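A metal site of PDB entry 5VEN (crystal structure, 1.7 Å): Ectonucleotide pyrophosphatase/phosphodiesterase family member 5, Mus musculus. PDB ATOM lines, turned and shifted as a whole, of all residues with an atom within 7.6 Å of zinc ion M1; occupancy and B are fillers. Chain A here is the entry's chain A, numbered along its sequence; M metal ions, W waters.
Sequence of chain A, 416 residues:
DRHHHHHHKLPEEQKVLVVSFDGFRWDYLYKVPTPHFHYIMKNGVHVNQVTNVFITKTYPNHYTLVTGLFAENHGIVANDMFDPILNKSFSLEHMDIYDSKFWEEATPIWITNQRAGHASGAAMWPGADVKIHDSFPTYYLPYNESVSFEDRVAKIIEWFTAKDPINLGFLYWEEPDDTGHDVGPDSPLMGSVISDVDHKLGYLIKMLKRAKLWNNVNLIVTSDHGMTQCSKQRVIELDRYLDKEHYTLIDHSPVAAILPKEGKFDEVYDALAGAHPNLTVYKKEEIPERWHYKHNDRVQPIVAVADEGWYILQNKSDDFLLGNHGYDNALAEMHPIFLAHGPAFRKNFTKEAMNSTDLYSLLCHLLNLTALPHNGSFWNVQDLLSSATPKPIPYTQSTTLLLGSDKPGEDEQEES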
ATOM      1  N   SER A  20      -7.396  -6.770 -15.759  1.00  0.00           N
ATOM      2  CA  SER A  20      -6.309  -6.776 -16.730  1.00  0.00           C
ATOM      3  C   SER A  20      -5.000  -7.032 -15.989  1.00  0.00           C
ATOM      4  O   SER A  20      -4.608  -6.228 -15.124  1.00  0.00           O
ATOM      5  CB  SER A  20      -6.234  -5.483 -17.509  1.00  0.00           C
ATOM      6  OG  SER A  20      -5.089  -5.514 -18.341  1.00  0.00           O
ATOM      7  N   PHE A  21      -4.361  -8.161 -16.308  1.00  0.00           N
ATOM      8  CA  PHE A  21      -2.969  -8.406 -15.931  1.00  0.00           C
ATOM      9  C   PHE A  21      -2.134  -7.965 -17.108  1.00  0.00           C
ATOM     10  O   PHE A  21      -2.187  -8.593 -18.167  1.00  0.00           O
ATOM     11  CB  PHE A  21      -2.745  -9.881 -15.599  1.00  0.00           C
ATOM     12  CG  PHE A  21      -3.455 -10.353 -14.375  1.00  0.00           C
ATOM     13  CD1 PHE A  21      -3.007  -9.957 -13.101  1.00  0.00           C
ATOM     14  CD2 PHE A  21      -4.554 -11.186 -14.458  1.00  0.00           C
ATOM     15  CE1 PHE A  21      -3.679 -10.413 -11.967  1.00  0.00           C
ATOM     16  CE2 PHE A  21      -5.186 -11.633 -13.317  1.00  0.00           C
ATOM     17  CZ  PHE A  21      -4.780 -11.230 -12.099  1.00  0.00           C
ATOM     18  N   ASP A  22      -1.406  -6.848 -16.949  1.00  0.00           N
ATOM     19  CA  ASP A  22      -0.693  -6.247 -18.082  1.00  0.00           C
ATOM     20  C   ASP A  22       0.265  -7.260 -18.701  1.00  0.00           C
ATOM     21  O   ASP A  22       0.996  -7.954 -17.995  1.00  0.00           O
ATOM     22  CB  ASP A  22       0.054  -5.000 -17.608  1.00  0.00           C
ATOM     23  CG  ASP A  22       0.327  -4.047 -18.745  1.00  0.00           C
ATOM     24  OD1 ASP A  22       0.978  -4.486 -19.716  1.00  0.00           O
ATOM     25  OD2 ASP A  22      -0.129  -2.891 -18.709  1.00  0.00           O
ATOM     26  N   GLY A  23       0.245  -7.331 -20.032  1.00  0.00           N
ATOM     27  CA  GLY A  23       1.248  -8.098 -20.753  1.00  0.00           C
ATOM     28  C   GLY A  23       1.106  -9.590 -20.563  1.00  0.00           C
ATOM     29  O   GLY A  23       2.115 -10.310 -20.597  1.00  0.00           O
ATOM     30  N   PHE A  24      -0.116 -10.092 -20.400  1.00  0.00           N
ATOM     31  CA  PHE A  24      -0.341 -11.531 -20.190  1.00  0.00           C
ATOM     32  C   PHE A  24      -0.611 -12.158 -21.543  1.00  0.00           C
ATOM     33  O   PHE A  24      -1.756 -12.169 -22.052  1.00  0.00           O
ATOM     34  CB  PHE A  24      -1.464 -11.783 -19.188  1.00  0.00           C
ATOM     35  CG  PHE A  24      -1.432 -13.153 -18.580  1.00  0.00           C
ATOM     36  CD1 PHE A  24      -1.601 -14.313 -19.358  1.00  0.00           C
ATOM     37  CD2 PHE A  24      -1.194 -13.299 -17.216  1.00  0.00           C
ATOM     38  CE1 PHE A  24      -1.590 -15.549 -18.769  1.00  0.00           C
ATOM     39  CE2 PHE A  24      -1.172 -14.569 -16.635  1.00  0.00           C
ATOM     40  CZ  PHE A  24      -1.354 -15.673 -17.435  1.00  0.00           C
ATOM     41  N   THR A  56       0.459  -2.277 -30.292  1.00  0.00           N
ATOM     42  CA  THR A  56       0.091  -3.238 -29.250  1.00  0.00           C
ATOM     43  C   THR A  56       0.779  -2.838 -27.939  1.00  0.00           C
ATOM     44  O   THR A  56       1.592  -3.580 -27.329  1.00  0.00           O
ATOM     45  CB  THR A  56       0.444  -4.668 -29.700  1.00  0.00           C
ATOM     46  OG1 THR A  56       1.813  -4.705 -30.107  1.00  0.00           O
ATOM     47  CG2 THR A  56      -0.494  -5.090 -30.818  1.00  0.00           C
ATOM     48  N   LYS A  57       0.444  -1.618 -27.485  1.00  0.00           N
ATOM     49  CA  LYS A  57       0.931  -1.000 -26.250  1.00  0.00           C
ATOM     50  C   LYS A  57      -0.234  -0.793 -25.271  1.00  0.00           C
ATOM     51  O   LYS A  57      -1.407  -0.961 -25.615  1.00  0.00           O
ATOM     52  CB  LYS A  57       1.611   0.365 -26.505  1.00  0.00           C
ATOM     53  CG  LYS A  57       2.876   0.352 -27.361  1.00  0.00           C
ATOM     54  CD  LYS A  57       4.081  -0.149 -26.660  1.00  0.00           C
ATOM     55  CE  LYS A  57       5.306   0.139 -27.501  1.00  0.00           C
ATOM     56  NZ  LYS A  57       6.481  -0.148 -26.720  1.00  0.00           N
ATOM     57  N   THR A  58       0.140  -0.413 -24.046  1.00  0.00           N
ATOM     58  CA  THR A  58      -0.767  -0.458 -22.902  1.00  0.00           C
ATOM     59  C   THR A  58      -1.911   0.555 -23.035  1.00  0.00           C
ATOM     60  O   THR A  58      -3.081   0.198 -22.881  1.00  0.00           O
ATOM     61  CB  THR A  58       0.006  -0.226 -21.610  1.00  0.00           C
ATOM     62  OG1 THR A  58       0.919  -1.345 -21.402  1.00  0.00           O
ATOM     63  CG2 THR A  58      -0.892  -0.162 -20.400  1.00  0.00           C
ATOM     64  N   TYR A  59      -1.588   1.825 -23.253  1.00  0.00           N
ATOM     65  CA  TYR A  59      -2.671   2.822 -23.197  1.00  0.00           C
ATOM     66  C   TYR A  59      -3.615   2.725 -24.394  1.00  0.00           C
ATOM     67  O   TYR A  59      -4.843   2.725 -24.183  1.00  0.00           O
ATOM     68  CB  TYR A  59      -2.089   4.219 -22.986  1.00  0.00           C
ATOM     69  CG  TYR A  59      -1.936   4.467 -21.495  1.00  0.00           C
ATOM     70  CD1 TYR A  59      -1.228   3.583 -20.686  1.00  0.00           C
ATOM     71  CD2 TYR A  59      -2.603   5.480 -20.877  1.00  0.00           C
ATOM     72  CE1 TYR A  59      -1.133   3.813 -19.295  1.00  0.00           C
ATOM     73  CE2 TYR A  59      -2.501   5.701 -19.547  1.00  0.00           C
ATOM     74  CZ  TYR A  59      -1.794   4.871 -18.748  1.00  0.00           C
ATOM     75  OH  TYR A  59      -1.775   5.148 -17.388  1.00  0.00           O
ATOM     76  N   ASN A  61      -4.432   0.001 -25.953  1.00  0.00           N
ATOM     77  CA  ASN A  61      -5.254  -1.189 -25.863  1.00  0.00           C
ATOM     78  C   ASN A  61      -6.229  -1.165 -24.704  1.00  0.00           C
ATOM     79  O   ASN A  61      -7.365  -1.651 -24.864  1.00  0.00           O
ATOM     80  CB  ASN A  61      -4.376  -2.441 -25.841  1.00  0.00           C
ATOM     81  CG  ASN A  61      -4.094  -2.897 -27.254  1.00  0.00           C
ATOM     82  OD1 ASN A  61      -4.932  -3.538 -27.882  1.00  0.00           O
ATOM     83  ND2 ASN A  61      -3.013  -2.405 -27.823  1.00  0.00           N
ATOM     84  N   HIS A  62      -5.858  -0.558 -23.575  1.00  0.00           N
ATOM     85  CA  HIS A  62      -6.840  -0.430 -22.497  1.00  0.00           C
ATOM     86  C   HIS A  62      -7.960   0.523 -22.905  1.00  0.00           C
ATOM     87  O   HIS A  62      -9.132   0.271 -22.599  1.00  0.00           O
ATOM     88  CB  HIS A  62      -6.203  -0.010 -21.194  1.00  0.00           C
ATOM     89  CG  HIS A  62      -5.520  -1.129 -20.458  1.00  0.00           C
ATOM     90  ND1 HIS A  62      -4.186  -1.395 -20.642  1.00  0.00           N
ATOM     91  CD2 HIS A  62      -5.976  -2.043 -19.554  1.00  0.00           C
ATOM     92  CE1 HIS A  62      -3.826  -2.420 -19.865  1.00  0.00           C
ATOM     93  NE2 HIS A  62      -4.897  -2.825 -19.200  1.00  0.00           N
ATOM     94  N   ASN A  79       1.655   5.310 -26.202  1.00  0.00           N
ATOM     95  CA  ASN A  79       1.957   5.747 -24.841  1.00  0.00           C
ATOM     96  C   ASN A  79       2.680   7.083 -24.828  1.00  0.00           C
ATOM     97  O   ASN A  79       2.721   7.733 -23.788  1.00  0.00           O
ATOM     98  CB  ASN A  79       2.840   4.726 -24.104  1.00  0.00           C
ATOM     99  CG  ASN A  79       2.191   3.403 -23.896  1.00  0.00           C
ATOM    100  OD1 ASN A  79       0.955   3.259 -23.866  1.00  0.00           O
ATOM    101  ND2 ASN A  79       3.027   2.392 -23.708  1.00  0.00           N
ATOM    102  N   LEU A  92       3.478   8.371 -21.004  1.00  0.00           N
ATOM    103  CA  LEU A  92       3.328   7.460 -19.868  1.00  0.00           C
ATOM    104  C   LEU A  92       4.548   7.485 -18.956  1.00  0.00           C
ATOM    105  O   LEU A  92       4.411   7.485 -17.722  1.00  0.00           O
ATOM    106  CB  LEU A  92       3.085   6.046 -20.383  1.00  0.00           C
ATOM    107  CG  LEU A  92       2.915   4.959 -19.352  1.00  0.00           C
ATOM    108  CD1 LEU A  92       1.822   5.331 -18.326  1.00  0.00           C
ATOM    109  CD2 LEU A  92       2.584   3.672 -20.098  1.00  0.00           C
ATOM    110  N   PRO A 126      -5.609   1.806 -16.431  1.00  0.00           N
ATOM    111  CA  PRO A 126      -5.065   2.916 -17.225  1.00  0.00           C
ATOM    112  C   PRO A 126      -6.134   3.883 -17.712  1.00  0.00           C
ATOM    113  O   PRO A 126      -7.104   3.482 -18.380  1.00  0.00           O
ATOM    114  CB  PRO A 126      -4.381   2.190 -18.408  1.00  0.00           C
ATOM    115  CG  PRO A 126      -3.936   0.951 -17.805  1.00  0.00           C
ATOM    116  CD  PRO A 126      -5.041   0.525 -16.855  1.00  0.00           C
ATOM    117  N   TYR A 172      -6.586  -3.656 -12.222  1.00  0.00           N
ATOM    118  CA  TYR A 172      -5.396  -3.693 -13.060  1.00  0.00           C
ATOM    119  C   TYR A 172      -4.179  -4.041 -12.213  1.00  0.00           C
ATOM    120  O   TYR A 172      -4.075  -3.622 -11.031  1.00  0.00           O
ATOM    121  CB  TYR A 172      -5.210  -2.352 -13.748  1.00  0.00           C
ATOM    122  CG  TYR A 172      -3.899  -2.173 -14.492  1.00  0.00           C
ATOM    123  CD1 TYR A 172      -3.698  -2.686 -15.779  1.00  0.00           C
ATOM    124  CD2 TYR A 172      -2.884  -1.421 -13.922  1.00  0.00           C
ATOM    125  CE1 TYR A 172      -2.511  -2.497 -16.446  1.00  0.00           C
ATOM    126  CE2 TYR A 172      -1.706  -1.181 -14.598  1.00  0.00           C
ATOM    127  CZ  TYR A 172      -1.516  -1.741 -15.846  1.00  0.00           C
ATOM    128  OH  TYR A 172      -0.337  -1.521 -16.482  1.00  0.00           O
ATOM    129  N   TRP A 173      -3.263  -4.803 -12.821  1.00  0.00           N
ATOM    130  CA  TRP A 173      -2.007  -5.208 -12.196  1.00  0.00           C
ATOM    131  C   TRP A 173      -0.914  -5.204 -13.267  1.00  0.00           C
ATOM    132  O   TRP A 173      -1.167  -5.538 -14.420  1.00  0.00           O
ATOM    133  CB  TRP A 173      -2.173  -6.595 -11.587  1.00  0.00           C
ATOM    134  CG  TRP A 173      -1.008  -7.076 -10.788  1.00  0.00           C
ATOM    135  CD1 TRP A 173      -0.203  -8.166 -11.042  1.00  0.00           C
ATOM    136  CD2 TRP A 173      -0.479  -6.466  -9.591  1.00  0.00           C
ATOM    137  NE1 TRP A 173       0.762  -8.277 -10.076  1.00  0.00           N
ATOM    138  CE2 TRP A 173       0.620  -7.253  -9.181  1.00  0.00           C
ATOM    139  CE3 TRP A 173      -0.833  -5.355  -8.830  1.00  0.00           C
ATOM    140  CZ2 TRP A 173       1.369  -6.945  -8.025  1.00  0.00           C
ATOM    141  CZ3 TRP A 173      -0.089  -5.067  -7.689  1.00  0.00           C
ATOM    142  CH2 TRP A 173       0.994  -5.851  -7.313  1.00  0.00           C
ATOM    143  N   GLU A 174       0.312  -4.797 -12.871  1.00  0.00           N
ATOM    144  CA  GLU A 174       1.369  -4.495 -13.819  1.00  0.00           C
ATOM    145  C   GLU A 174       2.179  -5.712 -14.260  1.00  0.00           C
ATOM    146  O   GLU A 174       3.033  -5.563 -15.135  1.00  0.00           O
ATOM    147  CB  GLU A 174       2.312  -3.487 -13.196  1.00  0.00           C
ATOM    148  CG  GLU A 174       1.684  -2.108 -12.960  1.00  0.00           C
ATOM    149  CD  GLU A 174       0.817  -1.992 -11.683  1.00  0.00           C
ATOM    150  OE1 GLU A 174       0.088  -0.983 -11.514  1.00  0.00           O
ATOM    151  OE2 GLU A 174       0.841  -2.882 -10.838  1.00  0.00           O
ATOM    152  N   ASP A 177       3.727  -8.148 -17.343  1.00  0.00           N
ATOM    153  CA  ASP A 177       4.400  -7.246 -18.280  1.00  0.00           C
ATOM    154  C   ASP A 177       5.781  -6.843 -17.772  1.00  0.00           C
ATOM    155  O   ASP A 177       6.764  -6.906 -18.532  1.00  0.00           O
ATOM    156  CB  ASP A 177       3.554  -6.002 -18.512  1.00  0.00           C
ATOM    157  CG  ASP A 177       4.250  -4.974 -19.388  1.00  0.00           C
ATOM    158  OD1 ASP A 177       4.219  -5.125 -20.614  1.00  0.00           O
ATOM    159  OD2 ASP A 177       4.855  -4.021 -18.798  1.00  0.00           O
ATOM    160  N   HIS A 181       9.408  -7.750 -19.680  1.00  0.00           N
ATOM    161  CA  HIS A 181      10.391  -6.810 -20.238  1.00  0.00           C
ATOM    162  C   HIS A 181      11.791  -7.086 -19.711  1.00  0.00           C
ATOM    163  O   HIS A 181      12.780  -7.062 -20.493  1.00  0.00           O
ATOM    164  CB  HIS A 181      10.023  -5.387 -19.850  1.00  0.00           C
ATOM    165  CG  HIS A 181       8.899  -4.811 -20.631  1.00  0.00           C
ATOM    166  ND1 HIS A 181       8.994  -4.575 -21.987  1.00  0.00           N
ATOM    167  CD2 HIS A 181       7.703  -4.313 -20.242  1.00  0.00           C
ATOM    168  CE1 HIS A 181       7.863  -4.015 -22.409  1.00  0.00           C
ATOM    169  NE2 HIS A 181       7.066  -3.846 -21.374  1.00  0.00           N
ATOM    170  N   SER A 223      -6.095  -8.993 -20.894  1.00  0.00           N
ATOM    171  CA  SER A 223      -4.874  -8.219 -20.891  1.00  0.00           C
ATOM    172  C   SER A 223      -4.914  -7.316 -22.105  1.00  0.00           C
ATOM    173  O   SER A 223      -5.841  -7.395 -22.913  1.00  0.00           O
ATOM    174  CB  SER A 223      -3.644  -9.150 -20.851  1.00  0.00           C
ATOM    175  OG  SER A 223      -2.439  -8.414 -20.750  1.00  0.00           O
ATOM    176  N   ASP A 224      -3.889  -6.490 -22.224  1.00  0.00           N
ATOM    177  CA  ASP A 224      -3.766  -5.517 -23.288  1.00  0.00           C
ATOM    178  C   ASP A 224      -2.922  -5.990 -24.476  1.00  0.00           C
ATOM    179  O   ASP A 224      -3.172  -5.575 -25.609  1.00  0.00           O
ATOM    180  CB  ASP A 224      -3.191  -4.220 -22.731  1.00  0.00           C
ATOM    181  CG  ASP A 224      -1.915  -4.365 -21.904  1.00  0.00           C
ATOM    182  OD1 ASP A 224      -1.525  -5.494 -21.493  1.00  0.00           O
ATOM    183  OD2 ASP A 224      -1.289  -3.289 -21.647  1.00  0.00           O
ATOM    184  N   HIS A 225      -1.979  -6.896 -24.229  1.00  0.00           N
ATOM    185  CA  HIS A 225      -1.046  -7.331 -25.268  1.00  0.00           C
ATOM    186  C   HIS A 225      -0.190  -8.432 -24.651  1.00  0.00           C
ATOM    187  O   HIS A 225      -0.226  -8.695 -23.433  1.00  0.00           O
ATOM    188  CB  HIS A 225      -0.127  -6.203 -25.748  1.00  0.00           C
ATOM    189  CG  HIS A 225       0.578  -5.539 -24.609  1.00  0.00           C
ATOM    190  ND1 HIS A 225       1.583  -6.156 -23.891  1.00  0.00           N
ATOM    191  CD2 HIS A 225       0.322  -4.359 -23.989  1.00  0.00           C
ATOM    192  CE1 HIS A 225       1.910  -5.384 -22.857  1.00  0.00           C
ATOM    193  NE2 HIS A 225       1.138  -4.294 -22.880  1.00  0.00           N
ATOM    194  N   GLY A 226       0.601  -9.059 -25.516  1.00  0.00           N
ATOM    195  CA  GLY A 226       1.595 -10.080 -25.118  1.00  0.00           C
ATOM    196  C   GLY A 226       2.978  -9.496 -25.008  1.00  0.00           C
ATOM    197  O   GLY A 226       3.195  -8.381 -24.521  1.00  0.00           O
ATOM    198  N   MET A 227       3.951 -10.257 -25.498  1.00  0.00           N
ATOM    199  CA  MET A 227       5.355  -9.947 -25.285  1.00  0.00           C
ATOM    200  C   MET A 227       6.164 -10.839 -26.232  1.00  0.00           C
ATOM    201  O   MET A 227       5.803 -11.997 -26.430  1.00  0.00           O
ATOM    202  CB  MET A 227       5.746 -10.207 -23.821  1.00  0.00           C
ATOM    203  CG  MET A 227       7.125  -9.669 -23.438  1.00  0.00           C
ATOM    204  SD  MET A 227       7.297  -7.885 -23.234  1.00  0.00           S
ATOM    205  CE  MET A 227       6.172  -7.611 -21.884  1.00  0.00           C
ATOM    206  N   HIS A 325       6.866  -5.303 -26.729  1.00  0.00           N
ATOM    207  CA  HIS A 325       5.620  -5.453 -27.456  1.00  0.00           C
ATOM    208  C   HIS A 325       5.352  -4.109 -28.136  1.00  0.00           C
ATOM    209  O   HIS A 325       6.097  -3.145 -27.973  1.00  0.00           O
ATOM    210  CB  HIS A 325       4.485  -5.860 -26.514  1.00  0.00           C
ATOM    211  CG  HIS A 325       4.376  -4.951 -25.351  1.00  0.00           C
ATOM    212  ND1 HIS A 325       3.564  -3.836 -25.352  1.00  0.00           N
ATOM    213  CD2 HIS A 325       5.027  -4.935 -24.153  1.00  0.00           C
ATOM    214  CE1 HIS A 325       3.688  -3.198 -24.199  1.00  0.00           C
ATOM    215  NE2 HIS A 325       4.601  -3.824 -23.459  1.00  0.00           N
HETATM  216 ZN    ZN M   1       0.617  -3.233 -21.219  1.00  0.00          ZN
HETATM  217 ZN    ZN M   2       5.082  -3.475 -21.504  1.00  0.00          ZN
HETATM  218  O   HOH W   1       3.036  -2.517 -20.766  1.00  0.00           O
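The backbone carbonyl oxygen (O) of Thr 58 is in hydrogen-bond range of a ring nitrogen (ND1) of His 62 (3.0 Å). The side-chain carboxylate of Asp 224 is in hydrogen-bond range of the backbone NH of Gly 23 (2.9 Å). The backbone carbonyl oxygen of Asp 22 is in hydrogen-bond range of the backbone NH of Asp 177 (2.8 Å). The side-chain hydroxyl of Tyr 172 sits at hydrogen-bond distance from the side-chain carboxylate of Asp 22 (2.6 Å). The backbone carbonyl oxygen of Trp 173 sits at hydrogen-bond distance from the backbone NH of Asp 22 (2.9 Å). A ring nitrogen (ND1) of His 225 lies close to a ring nitrogen (ND1) of His 325 (3.4 Å). O of His 225 sits at hydrogen-bond distance from OG of Ser 223 (3.5 Å). The backbone NH (N) of Phe 24 lies within hydrogen-bond range of the backbone carbonyl oxygen (O) of His 225 (3.3 Å).
The nearest printed residue that does not touch zinc ion M1 is Asp 177 (4.1 Å).
Zinc ion M1 is bound by the side-chain hydroxyl (OG1) of Thr 58 (1.9 Å), the side-chain carboxylate (OD2) of Asp 224 (2.0 Å), the side-chain carboxylate (OD1) of Asp 22 (2.0 Å), a ring nitrogen (NE2) of His 225 (2.0 Å) and water W1 (2.6 Å). Slightly farther from zinc ion M1 lies OD2 of Asp 22 (2.6 Å).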
